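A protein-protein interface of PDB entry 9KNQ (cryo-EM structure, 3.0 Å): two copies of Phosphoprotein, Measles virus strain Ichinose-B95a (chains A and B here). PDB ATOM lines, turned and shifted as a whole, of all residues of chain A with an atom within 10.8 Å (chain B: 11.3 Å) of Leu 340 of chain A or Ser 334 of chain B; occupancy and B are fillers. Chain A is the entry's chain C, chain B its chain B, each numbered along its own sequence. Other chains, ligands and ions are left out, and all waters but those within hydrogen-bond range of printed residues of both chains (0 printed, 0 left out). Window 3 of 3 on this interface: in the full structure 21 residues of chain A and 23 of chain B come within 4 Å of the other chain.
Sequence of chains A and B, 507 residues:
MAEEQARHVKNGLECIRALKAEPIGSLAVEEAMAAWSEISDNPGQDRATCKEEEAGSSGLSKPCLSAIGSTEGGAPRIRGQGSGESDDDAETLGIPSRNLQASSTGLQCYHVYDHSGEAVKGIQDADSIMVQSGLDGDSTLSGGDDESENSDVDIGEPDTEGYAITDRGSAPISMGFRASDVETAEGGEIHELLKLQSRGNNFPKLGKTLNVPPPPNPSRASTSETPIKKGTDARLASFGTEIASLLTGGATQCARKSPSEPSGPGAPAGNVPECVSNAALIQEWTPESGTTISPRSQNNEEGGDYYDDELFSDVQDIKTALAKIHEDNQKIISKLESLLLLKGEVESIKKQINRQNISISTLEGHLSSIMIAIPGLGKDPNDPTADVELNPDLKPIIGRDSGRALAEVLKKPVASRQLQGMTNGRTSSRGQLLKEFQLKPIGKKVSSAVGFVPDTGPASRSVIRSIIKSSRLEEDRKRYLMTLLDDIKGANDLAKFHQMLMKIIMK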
ATOM      1  N   LYS A 331      -1.637  24.970  37.881  1.00  0.00           N
ATOM      2  CA  LYS A 331      -2.951  24.488  37.470  1.00  0.00           C
ATOM      3  C   LYS A 331      -3.103  24.577  35.957  1.00  0.00           C
ATOM      4  O   LYS A 331      -3.651  23.665  35.328  1.00  0.00           O
ATOM      5  CB  LYS A 331      -4.042  25.292  38.179  1.00  0.00           C
ATOM      6  CG  LYS A 331      -5.270  24.491  38.597  1.00  0.00           C
ATOM      7  CD  LYS A 331      -6.135  24.023  37.442  1.00  0.00           C
ATOM      8  CE  LYS A 331      -7.585  23.920  37.897  1.00  0.00           C
ATOM      9  NZ  LYS A 331      -8.430  23.114  36.979  1.00  0.00           N
ATOM     10  N   ILE A 332      -2.608  25.665  35.359  1.00  0.00           N
ATOM     11  CA  ILE A 332      -2.603  25.795  33.902  1.00  0.00           C
ATOM     12  C   ILE A 332      -1.863  24.621  33.272  1.00  0.00           C
ATOM     13  O   ILE A 332      -2.376  23.949  32.366  1.00  0.00           O
ATOM     14  CB  ILE A 332      -1.974  27.137  33.483  1.00  0.00           C
ATOM     15  CG1 ILE A 332      -2.905  28.304  33.815  1.00  0.00           C
ATOM     16  CG2 ILE A 332      -1.644  27.130  32.000  1.00  0.00           C
ATOM     17  CD1 ILE A 332      -4.113  28.400  32.911  1.00  0.00           C
ATOM     18  N   ILE A 333      -0.642  24.356  33.751  1.00  0.00           N
ATOM     19  CA  ILE A 333       0.183  23.298  33.171  1.00  0.00           C
ATOM     20  C   ILE A 333      -0.509  21.948  33.304  1.00  0.00           C
ATOM     21  O   ILE A 333      -0.598  21.178  32.338  1.00  0.00           O
ATOM     22  CB  ILE A 333       1.577  23.286  33.827  1.00  0.00           C
ATOM     23  CG1 ILE A 333       2.446  24.404  33.254  1.00  0.00           C
ATOM     24  CG2 ILE A 333       2.251  21.935  33.633  1.00  0.00           C
ATOM     25  CD1 ILE A 333       2.716  24.264  31.777  1.00  0.00           C
ATOM     26  N   SER A 334      -1.023  21.650  34.501  1.00  0.00           N
ATOM     27  CA  SER A 334      -1.637  20.350  34.750  1.00  0.00           C
ATOM     28  C   SER A 334      -2.893  20.151  33.907  1.00  0.00           C
ATOM     29  O   SER A 334      -3.063  19.106  33.266  1.00  0.00           O
ATOM     30  CB  SER A 334      -1.960  20.199  36.238  1.00  0.00           C
ATOM     31  OG  SER A 334      -0.959  20.799  37.045  1.00  0.00           O
ATOM     32  N   LYS A 335      -3.785  21.141  33.889  1.00  0.00           N
ATOM     33  CA  LYS A 335      -5.048  20.994  33.179  1.00  0.00           C
ATOM     34  C   LYS A 335      -4.925  21.266  31.685  1.00  0.00           C
ATOM     35  O   LYS A 335      -5.917  21.125  30.963  1.00  0.00           O
ATOM     36  CB  LYS A 335      -6.107  21.906  33.799  1.00  0.00           C
ATOM     37  CG  LYS A 335      -7.069  21.172  34.717  1.00  0.00           C
ATOM     38  CD  LYS A 335      -6.320  20.346  35.746  1.00  0.00           C
ATOM     39  CE  LYS A 335      -7.274  19.548  36.607  1.00  0.00           C
ATOM     40  NZ  LYS A 335      -6.563  18.907  37.743  1.00  0.00           N
ATOM     41  N   LEU A 336      -3.743  21.650  31.207  1.00  0.00           N
ATOM     42  CA  LEU A 336      -3.464  21.574  29.780  1.00  0.00           C
ATOM     43  C   LEU A 336      -2.906  20.204  29.404  1.00  0.00           C
ATOM     44  O   LEU A 336      -3.396  19.568  28.460  1.00  0.00           O
ATOM     45  CB  LEU A 336      -2.486  22.678  29.367  1.00  0.00           C
ATOM     46  CG  LEU A 336      -3.030  23.825  28.510  1.00  0.00           C
ATOM     47  CD1 LEU A 336      -3.976  24.704  29.312  1.00  0.00           C
ATOM     48  CD2 LEU A 336      -1.888  24.646  27.927  1.00  0.00           C
ATOM     49  N   GLU A 337      -1.894  19.736  30.146  1.00  0.00           N
ATOM     50  CA  GLU A 337      -1.254  18.469  29.812  1.00  0.00           C
ATOM     51  C   GLU A 337      -2.232  17.307  29.923  1.00  0.00           C
ATOM     52  O   GLU A 337      -2.192  16.383  29.102  1.00  0.00           O
ATOM     53  CB  GLU A 337      -0.031  18.238  30.704  1.00  0.00           C
ATOM     54  CG  GLU A 337      -0.325  18.121  32.192  1.00  0.00           C
ATOM     55  CD  GLU A 337      -0.579  16.695  32.637  1.00  0.00           C
ATOM     56  OE1 GLU A 337       0.244  15.812  32.317  1.00  0.00           O
ATOM     57  OE2 GLU A 337      -1.610  16.457  33.300  1.00  0.00           O
ATOM     58  N   SER A 338      -3.131  17.343  30.913  1.00  0.00           N
ATOM     59  CA  SER A 338      -4.075  16.245  31.103  1.00  0.00           C
ATOM     60  C   SER A 338      -4.854  15.959  29.826  1.00  0.00           C
ATOM     61  O   SER A 338      -4.776  14.861  29.263  1.00  0.00           O
ATOM     62  CB  SER A 338      -5.028  16.569  32.256  1.00  0.00           C
ATOM     63  OG  SER A 338      -6.329  16.060  32.009  1.00  0.00           O
ATOM     64  N   LEU A 339      -5.608  16.949  29.350  1.00  0.00           N
ATOM     65  CA  LEU A 339      -6.408  16.753  28.148  1.00  0.00           C
ATOM     66  C   LEU A 339      -5.541  16.578  26.909  1.00  0.00           C
ATOM     67  O   LEU A 339      -5.860  15.753  26.040  1.00  0.00           O
ATOM     68  CB  LEU A 339      -7.373  17.925  27.970  1.00  0.00           C
ATOM     69  CG  LEU A 339      -8.503  18.028  29.001  1.00  0.00           C
ATOM     70  CD1 LEU A 339      -8.976  16.645  29.435  1.00  0.00           C
ATOM     71  CD2 LEU A 339      -8.074  18.847  30.201  1.00  0.00           C
ATOM     72  N   LEU A 340      -4.429  17.314  26.815  1.00  0.00           N
ATOM     73  CA  LEU A 340      -3.647  17.274  25.589  1.00  0.00           C
ATOM     74  C   LEU A 340      -2.817  16.001  25.478  1.00  0.00           C
ATOM     75  O   LEU A 340      -2.195  15.774  24.436  1.00  0.00           O
ATOM     76  CB  LEU A 340      -2.778  18.525  25.496  1.00  0.00           C
ATOM     77  CG  LEU A 340      -3.593  19.814  25.308  1.00  0.00           C
ATOM     78  CD1 LEU A 340      -2.816  20.860  24.550  1.00  0.00           C
ATOM     79  CD2 LEU A 340      -4.920  19.546  24.599  1.00  0.00           C
ATOM     80  N   LEU A 341      -2.792  15.170  26.524  1.00  0.00           N
ATOM     81  CA  LEU A 341      -2.295  13.807  26.381  1.00  0.00           C
ATOM     82  C   LEU A 341      -3.407  12.768  26.318  1.00  0.00           C
ATOM     83  O   LEU A 341      -3.252  11.761  25.620  1.00  0.00           O
ATOM     84  CB  LEU A 341      -1.329  13.447  27.521  1.00  0.00           C
ATOM     85  CG  LEU A 341      -1.790  13.279  28.972  1.00  0.00           C
ATOM     86  CD1 LEU A 341      -2.157  11.833  29.278  1.00  0.00           C
ATOM     87  CD2 LEU A 341      -0.700  13.751  29.927  1.00  0.00           C
ATOM     88  N   LEU A 342      -4.525  12.976  27.022  1.00  0.00           N
ATOM     89  CA  LEU A 342      -5.638  12.032  26.963  1.00  0.00           C
ATOM     90  C   LEU A 342      -6.498  12.206  25.714  1.00  0.00           C
ATOM     91  O   LEU A 342      -7.557  11.575  25.612  1.00  0.00           O
ATOM     92  CB  LEU A 342      -6.506  12.155  28.219  1.00  0.00           C
ATOM     93  CG  LEU A 342      -5.952  11.471  29.475  1.00  0.00           C
ATOM     94  CD1 LEU A 342      -6.123  12.345  30.712  1.00  0.00           C
ATOM     95  CD2 LEU A 342      -6.603  10.110  29.676  1.00  0.00           C
ATOM     96  N   LYS A 343      -6.069  13.063  24.788  1.00  0.00           N
ATOM     97  CA  LYS A 343      -6.678  13.223  23.469  1.00  0.00           C
ATOM     98  C   LYS A 343      -7.031  11.914  22.753  1.00  0.00           C
ATOM     99  O   LYS A 343      -7.942  11.898  21.918  1.00  0.00           O
ATOM    100  CB  LYS A 343      -5.737  14.059  22.594  1.00  0.00           C
ATOM    101  CG  LYS A 343      -6.112  14.143  21.125  1.00  0.00           C
ATOM    102  CD  LYS A 343      -5.047  14.871  20.328  1.00  0.00           C
ATOM    103  CE  LYS A 343      -5.239  14.655  18.837  1.00  0.00           C
ATOM    104  NZ  LYS A 343      -4.237  15.412  18.040  1.00  0.00           N
ATOM    105  N   GLY A 344      -6.343  10.814  23.065  1.00  0.00           N
ATOM    106  CA  GLY A 344      -6.472   9.560  22.331  1.00  0.00           C
ATOM    107  C   GLY A 344      -7.871   9.048  22.018  1.00  0.00           C
ATOM    108  O   GLY A 344      -8.050   8.158  21.170  1.00  0.00           O
ATOM    109  N   GLU A 345      -8.882   9.589  22.701  1.00  0.00           N
ATOM    110  CA  GLU A 345     -10.244   9.181  22.388  1.00  0.00           C
ATOM    111  C   GLU A 345     -10.640   9.530  20.956  1.00  0.00           C
ATOM    112  O   GLU A 345     -11.538   8.884  20.404  1.00  0.00           O
ATOM    113  CB  GLU A 345     -11.238   9.768  23.398  1.00  0.00           C
ATOM    114  CG  GLU A 345     -11.082  11.236  23.773  1.00  0.00           C
ATOM    115  CD  GLU A 345     -11.287  12.181  22.611  1.00  0.00           C
ATOM    116  OE1 GLU A 345     -10.353  12.941  22.302  1.00  0.00           O
ATOM    117  OE2 GLU A 345     -12.363  12.142  21.981  1.00  0.00           O
ATOM    118  N   VAL A 346      -9.968  10.496  20.324  1.00  0.00           N
ATOM    119  CA  VAL A 346     -10.270  10.801  18.928  1.00  0.00           C
ATOM    120  C   VAL A 346      -9.876   9.632  18.024  1.00  0.00           C
ATOM    121  O   VAL A 346     -10.667   9.187  17.184  1.00  0.00           O
ATOM    122  CB  VAL A 346      -9.599  12.120  18.495  1.00  0.00           C
ATOM    123  CG1 VAL A 346     -10.178  13.295  19.266  1.00  0.00           C
ATOM    124  CG2 VAL A 346      -8.091  12.070  18.695  1.00  0.00           C
ATOM    125  N   ASN B 329       5.240  31.209  27.493  1.00  0.00           N
ATOM    126  CA  ASN B 329       6.451  30.606  28.037  1.00  0.00           C
ATOM    127  C   ASN B 329       6.429  29.099  27.802  1.00  0.00           C
ATOM    128  O   ASN B 329       7.236  28.568  27.039  1.00  0.00           O
ATOM    129  CB  ASN B 329       6.581  30.923  29.531  1.00  0.00           C
ATOM    130  CG  ASN B 329       7.925  30.505  30.109  1.00  0.00           C
ATOM    131  OD1 ASN B 329       8.342  29.354  29.985  1.00  0.00           O
ATOM    132  ND2 ASN B 329       8.608  31.448  30.746  1.00  0.00           N
ATOM    133  N   GLN B 330       5.498  28.415  28.467  1.00  0.00           N
ATOM    134  CA  GLN B 330       5.338  26.973  28.323  1.00  0.00           C
ATOM    135  C   GLN B 330       4.041  26.579  27.633  1.00  0.00           C
ATOM    136  O   GLN B 330       3.955  25.474  27.086  1.00  0.00           O
ATOM    137  CB  GLN B 330       5.394  26.292  29.695  1.00  0.00           C
ATOM    138  CG  GLN B 330       6.561  26.730  30.562  1.00  0.00           C
ATOM    139  CD  GLN B 330       6.193  27.842  31.524  1.00  0.00           C
ATOM    140  OE1 GLN B 330       5.068  28.342  31.512  1.00  0.00           O
ATOM    141  NE2 GLN B 330       7.143  28.236  32.363  1.00  0.00           N
ATOM    142  N   LYS B 331       3.034  27.453  27.646  1.00  0.00           N
ATOM    143  CA  LYS B 331       1.723  27.095  27.116  1.00  0.00           C
ATOM    144  C   LYS B 331       1.690  27.127  25.594  1.00  0.00           C
ATOM    145  O   LYS B 331       0.844  26.464  24.982  1.00  0.00           O
ATOM    146  CB  LYS B 331       0.662  28.036  27.688  1.00  0.00           C
ATOM    147  CG  LYS B 331       0.897  29.507  27.359  1.00  0.00           C
ATOM    148  CD  LYS B 331      -0.087  30.016  26.314  1.00  0.00           C
ATOM    149  CE  LYS B 331       0.114  31.498  26.033  1.00  0.00           C
ATOM    150  NZ  LYS B 331      -0.834  32.002  25.001  1.00  0.00           N
ATOM    151  N   ILE B 332       2.591  27.890  24.971  1.00  0.00           N
ATOM    152  CA  ILE B 332       2.489  28.173  23.539  1.00  0.00           C
ATOM    153  C   ILE B 332       2.475  26.882  22.730  1.00  0.00           C
ATOM    154  O   ILE B 332       1.523  26.601  21.992  1.00  0.00           O
ATOM    155  CB  ILE B 332       3.635  29.098  23.093  1.00  0.00           C
ATOM    156  CG1 ILE B 332       3.554  30.439  23.821  1.00  0.00           C
ATOM    157  CG2 ILE B 332       3.598  29.294  21.588  1.00  0.00           C
ATOM    158  CD1 ILE B 332       4.680  31.386  23.477  1.00  0.00           C
ATOM    159  N   ILE B 333       3.538  26.084  22.859  1.00  0.00           N
ATOM    160  CA  ILE B 333       3.708  24.892  22.026  1.00  0.00           C
ATOM    161  C   ILE B 333       2.485  23.992  22.130  1.00  0.00           C
ATOM    162  O   ILE B 333       1.783  23.735  21.142  1.00  0.00           O
ATOM    163  CB  ILE B 333       4.981  24.132  22.439  1.00  0.00           C
ATOM    164  CG1 ILE B 333       6.165  25.088  22.567  1.00  0.00           C
ATOM    165  CG2 ILE B 333       5.290  23.017  21.449  1.00  0.00           C
ATOM    166  CD1 ILE B 333       6.961  24.898  23.846  1.00  0.00           C
ATOM    167  N   SER B 334       2.214  23.515  23.345  1.00  0.00           N
ATOM    168  CA  SER B 334       1.168  22.526  23.561  1.00  0.00           C
ATOM    169  C   SER B 334      -0.202  23.077  23.180  1.00  0.00           C
ATOM    170  O   SER B 334      -0.940  22.451  22.406  1.00  0.00           O
ATOM    171  CB  SER B 334       1.204  22.071  25.021  1.00  0.00           C
ATOM    172  OG  SER B 334      -0.081  21.765  25.512  1.00  0.00           O
ATOM    173  N   LYS B 335      -0.560  24.251  23.715  1.00  0.00           N
ATOM    174  CA  LYS B 335      -1.853  24.856  23.417  1.00  0.00           C
ATOM    175  C   LYS B 335      -2.064  25.001  21.915  1.00  0.00           C
ATOM    176  O   LYS B 335      -3.029  24.465  21.359  1.00  0.00           O
ATOM    177  CB  LYS B 335      -1.955  26.215  24.117  1.00  0.00           C
ATOM    178  CG  LYS B 335      -2.993  27.161  23.525  1.00  0.00           C
ATOM    179  CD  LYS B 335      -4.159  27.375  24.476  1.00  0.00           C
ATOM    180  CE  LYS B 335      -3.755  28.260  25.643  1.00  0.00           C
ATOM    181  NZ  LYS B 335      -4.937  28.728  26.412  1.00  0.00           N
ATOM    182  N   LEU B 336      -1.156  25.709  21.236  1.00  0.00           N
ATOM    183  CA  LEU B 336      -1.345  25.988  19.817  1.00  0.00           C
ATOM    184  C   LEU B 336      -1.412  24.696  19.011  1.00  0.00           C
ATOM    185  O   LEU B 336      -2.332  24.506  18.205  1.00  0.00           O
ATOM    186  CB  LEU B 336      -0.218  26.898  19.317  1.00  0.00           C
ATOM    187  CG  LEU B 336      -0.363  27.708  18.017  1.00  0.00           C
ATOM    188  CD1 LEU B 336       0.777  28.712  17.904  1.00  0.00           C
ATOM    189  CD2 LEU B 336      -0.422  26.845  16.761  1.00  0.00           C
ATOM    190  N   GLU B 337      -0.460  23.782  19.228  1.00  0.00           N
ATOM    191  CA  GLU B 337      -0.415  22.560  18.432  1.00  0.00           C
ATOM    192  C   GLU B 337      -1.670  21.714  18.629  1.00  0.00           C
ATOM    193  O   GLU B 337      -2.407  21.439  17.670  1.00  0.00           O
ATOM    194  CB  GLU B 337       0.839  21.758  18.782  1.00  0.00           C
ATOM    195  CG  GLU B 337       1.958  21.879  17.761  1.00  0.00           C
ATOM    196  CD  GLU B 337       1.608  21.257  16.420  1.00  0.00           C
ATOM    197  OE1 GLU B 337       0.686  20.415  16.369  1.00  0.00           O
ATOM    198  OE2 GLU B 337       2.263  21.610  15.417  1.00  0.00           O
ATOM    199  N   SER B 338      -1.920  21.271  19.865  1.00  0.00           N
ATOM    200  CA  SER B 338      -3.032  20.371  20.128  1.00  0.00           C
ATOM    201  C   SER B 338      -4.360  21.105  20.274  1.00  0.00           C
ATOM    202  O   SER B 338      -5.337  20.511  20.743  1.00  0.00           O
ATOM    203  CB  SER B 338      -2.743  19.523  21.366  1.00  0.00           C
ATOM    204  OG  SER B 338      -1.937  18.405  21.035  1.00  0.00           O
ATOM    205  N   LEU B 339      -4.412  22.382  19.899  1.00  0.00           N
ATOM    206  CA  LEU B 339      -5.673  23.041  19.598  1.00  0.00           C
ATOM    207  C   LEU B 339      -5.900  23.203  18.107  1.00  0.00           C
ATOM    208  O   LEU B 339      -7.053  23.259  17.670  1.00  0.00           O
ATOM    209  CB  LEU B 339      -5.730  24.418  20.271  1.00  0.00           C
ATOM    210  CG  LEU B 339      -6.382  24.525  21.654  1.00  0.00           C
ATOM    211  CD1 LEU B 339      -7.902  24.548  21.542  1.00  0.00           C
ATOM    212  CD2 LEU B 339      -5.927  23.405  22.582  1.00  0.00           C
ATOM    213  N   LEU B 340      -4.824  23.277  17.319  1.00  0.00           N
ATOM    214  CA  LEU B 340      -4.965  23.324  15.868  1.00  0.00           C
ATOM    215  C   LEU B 340      -5.337  21.955  15.308  1.00  0.00           C
ATOM    216  O   LEU B 340      -6.142  21.857  14.376  1.00  0.00           O
ATOM    217  CB  LEU B 340      -3.669  23.840  15.240  1.00  0.00           C
ATOM    218  CG  LEU B 340      -3.751  24.722  13.989  1.00  0.00           C
ATOM    219  CD1 LEU B 340      -2.381  25.297  13.668  1.00  0.00           C
ATOM    220  CD2 LEU B 340      -4.294  23.957  12.796  1.00  0.00           C
ATOM    221  N   LEU B 341      -4.756  20.881  15.859  1.00  0.00           N
ATOM    222  CA  LEU B 341      -5.042  19.550  15.314  1.00  0.00           C
ATOM    223  C   LEU B 341      -6.504  19.155  15.515  1.00  0.00           C
ATOM    224  O   LEU B 341      -7.150  18.632  14.590  1.00  0.00           O
ATOM    225  CB  LEU B 341      -4.125  18.499  15.942  1.00  0.00           C
ATOM    226  CG  LEU B 341      -2.647  18.840  16.117  1.00  0.00           C
ATOM    227  CD1 LEU B 341      -1.929  17.757  16.911  1.00  0.00           C
ATOM    228  CD2 LEU B 341      -1.975  19.062  14.768  1.00  0.00           C
ATOM    229  N   LEU B 342      -7.038  19.398  16.716  1.00  0.00           N
ATOM    230  CA  LEU B 342      -8.418  19.032  17.013  1.00  0.00           C
ATOM    231  C   LEU B 342      -9.396  19.681  16.043  1.00  0.00           C
ATOM    232  O   LEU B 342     -10.468  19.123  15.792  1.00  0.00           O
ATOM    233  CB  LEU B 342      -8.765  19.412  18.452  1.00  0.00           C
ATOM    234  CG  LEU B 342      -7.821  18.921  19.552  1.00  0.00           C
ATOM    235  CD1 LEU B 342      -8.410  19.188  20.930  1.00  0.00           C
ATOM    236  CD2 LEU B 342      -7.532  17.443  19.380  1.00  0.00           C
ATOM    237  N   LYS B 343      -9.028  20.829  15.467  1.00  0.00           N
ATOM    238  CA  LYS B 343      -9.878  21.496  14.487  1.00  0.00           C
ATOM    239  C   LYS B 343     -10.245  20.545  13.353  1.00  0.00           C
ATOM    240  O   LYS B 343     -11.409  20.129  13.208  1.00  0.00           O
ATOM    241  CB  LYS B 343      -9.133  22.702  13.910  1.00  0.00           C
ATOM    242  CG  LYS B 343      -8.943  23.909  14.821  1.00  0.00           C
ATOM    243  CD  LYS B 343     -10.232  24.506  15.336  1.00  0.00           C
ATOM    244  CE  LYS B 343      -9.929  25.471  16.470  1.00  0.00           C
ATOM    245  NZ  LYS B 343     -10.872  25.354  17.612  1.00  0.00           N
ATOM    246  N   VAL B 346     -11.960  17.042  14.443  1.00  0.00           N
ATOM    247  CA  VAL B 346     -13.389  17.023  14.730  1.00  0.00           C
ATOM    248  C   VAL B 346     -14.197  17.318  13.474  1.00  0.00           C
ATOM    249  O   VAL B 346     -15.255  16.714  13.253  1.00  0.00           O
ATOM    250  CB  VAL B 346     -13.737  17.987  15.884  1.00  0.00           C
ATOM    251  CG1 VAL B 346     -12.923  17.648  17.125  1.00  0.00           C
ATOM    252  CG2 VAL B 346     -13.541  19.446  15.483  1.00  0.00           C
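Leu 340 of chain A touches Ser 334 of chain B, but with the chains exchanged Ser 334 of chain A does not touch Leu 340 of chain B (16.6 Å).
Leu 340 of chain A touches Ser 338 of chain B, but with the chains exchanged Ser 338 of chain A does not touch Leu 340 of chain B (14.5 Å).
Lys 343 of chain A touches Leu 341 of chain B, but with the chains exchanged Leu 341 of chain A does not touch Lys 343 of chain B (13.9 Å).
Lys 343 of chain A touches Leu 342 of chain B, but with the chains exchanged Leu 342 of chain A does not touch Lys 343 of chain B (13.6 Å).
Positions printed for both chains: 331, 332, 333, 334, 335, 336, 337, 338, 339, 340, 341, 342, 343 and 346.
Of the 5 pairs that touch across the chains among the printed residues, none has its exchanged pair printed and touching as well.
Of the printed residues of chain B, Ile 333 of chain A touches Gln 330 (3.95 Å).
No residue of chain B comes within 4 Å of Leu 336 of chain A.
No residue of chain B comes within 4 Å of Leu 339 of chain A.
Printed residues of chain B within 4 Å of Leu 340 of chain A: Ser 334 and Ser 338.
Printed residues of chain B within 4 Å of Lys 343 of chain A: Leu 341 (3.5 Å) and Leu 342 (3.7 Å).
Printed residues of chain A within 4 Å of Gln 330 of chain B: Ile 333.
No residue of chain A comes within 4 Å of Ile 333 of chain B.
Glu 337 of chain B touches none of the printed residues of chain A.
Of chain A, only Leu 340 comes within 4 Å of Ser 338 of chain B.
Printed residues of chain A within 4 Å of Leu 341 of chain B: Lys 343.
Of the printed residues of chain A, Leu 342 of chain B touches Lys 343.
The nearest residue of chain B that does not touch Leu 340 of chain A is Lys 335 of chain B (4.2 Å).
The nearest residue of chain A that does not touch Ser 334 of chain B is Leu 336 of chain A (4.2 Å).
The nearest printed residue of chain A that does not touch Gln 330 of chain B is Leu 336 of chain A (6.0 Å).
Among the printed residues, merely in contact across the chains: Ile 333 of chain A with Gln 330 of chain B, Leu 340 of chain A with Ser 334 of chain B, Leu 340 of chain A with Ser 338 of chain B, Lys 343 of chain A with Leu 341 of chain B and Lys 343 of chain A with Leu 342 of chain B.
Printed residues of chain B that touch a printed residue of chain A: Gln 330, Ser 334, Ser 338, Leu 341 and Leu 342.
Hydrophobic or aromatic side chains of chain B within 4 Å of the printed part of chain A: Leu 341 and Leu 342.
Printed residues of chain A that touch a printed residue of chain B: Ile 333, Leu 340 and Lys 343.
Hydrophobic or aromatic side chains of chain A that line the printed part of chain B: Ile 333 and Leu 340.
Among the printed residues, no Asp or Glu carboxylate lies within 4 Å of a Lys or Arg side-chain nitrogen of the other chain.
NE2 of Gln 330 of chain B sits at hydrogen-bond distance from OD1 of Asn 329 of chain B (2.9 Å).
O of Lys 343 of chain A lies close to OE1 of Glu 345 of chain A (2.7 Å).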
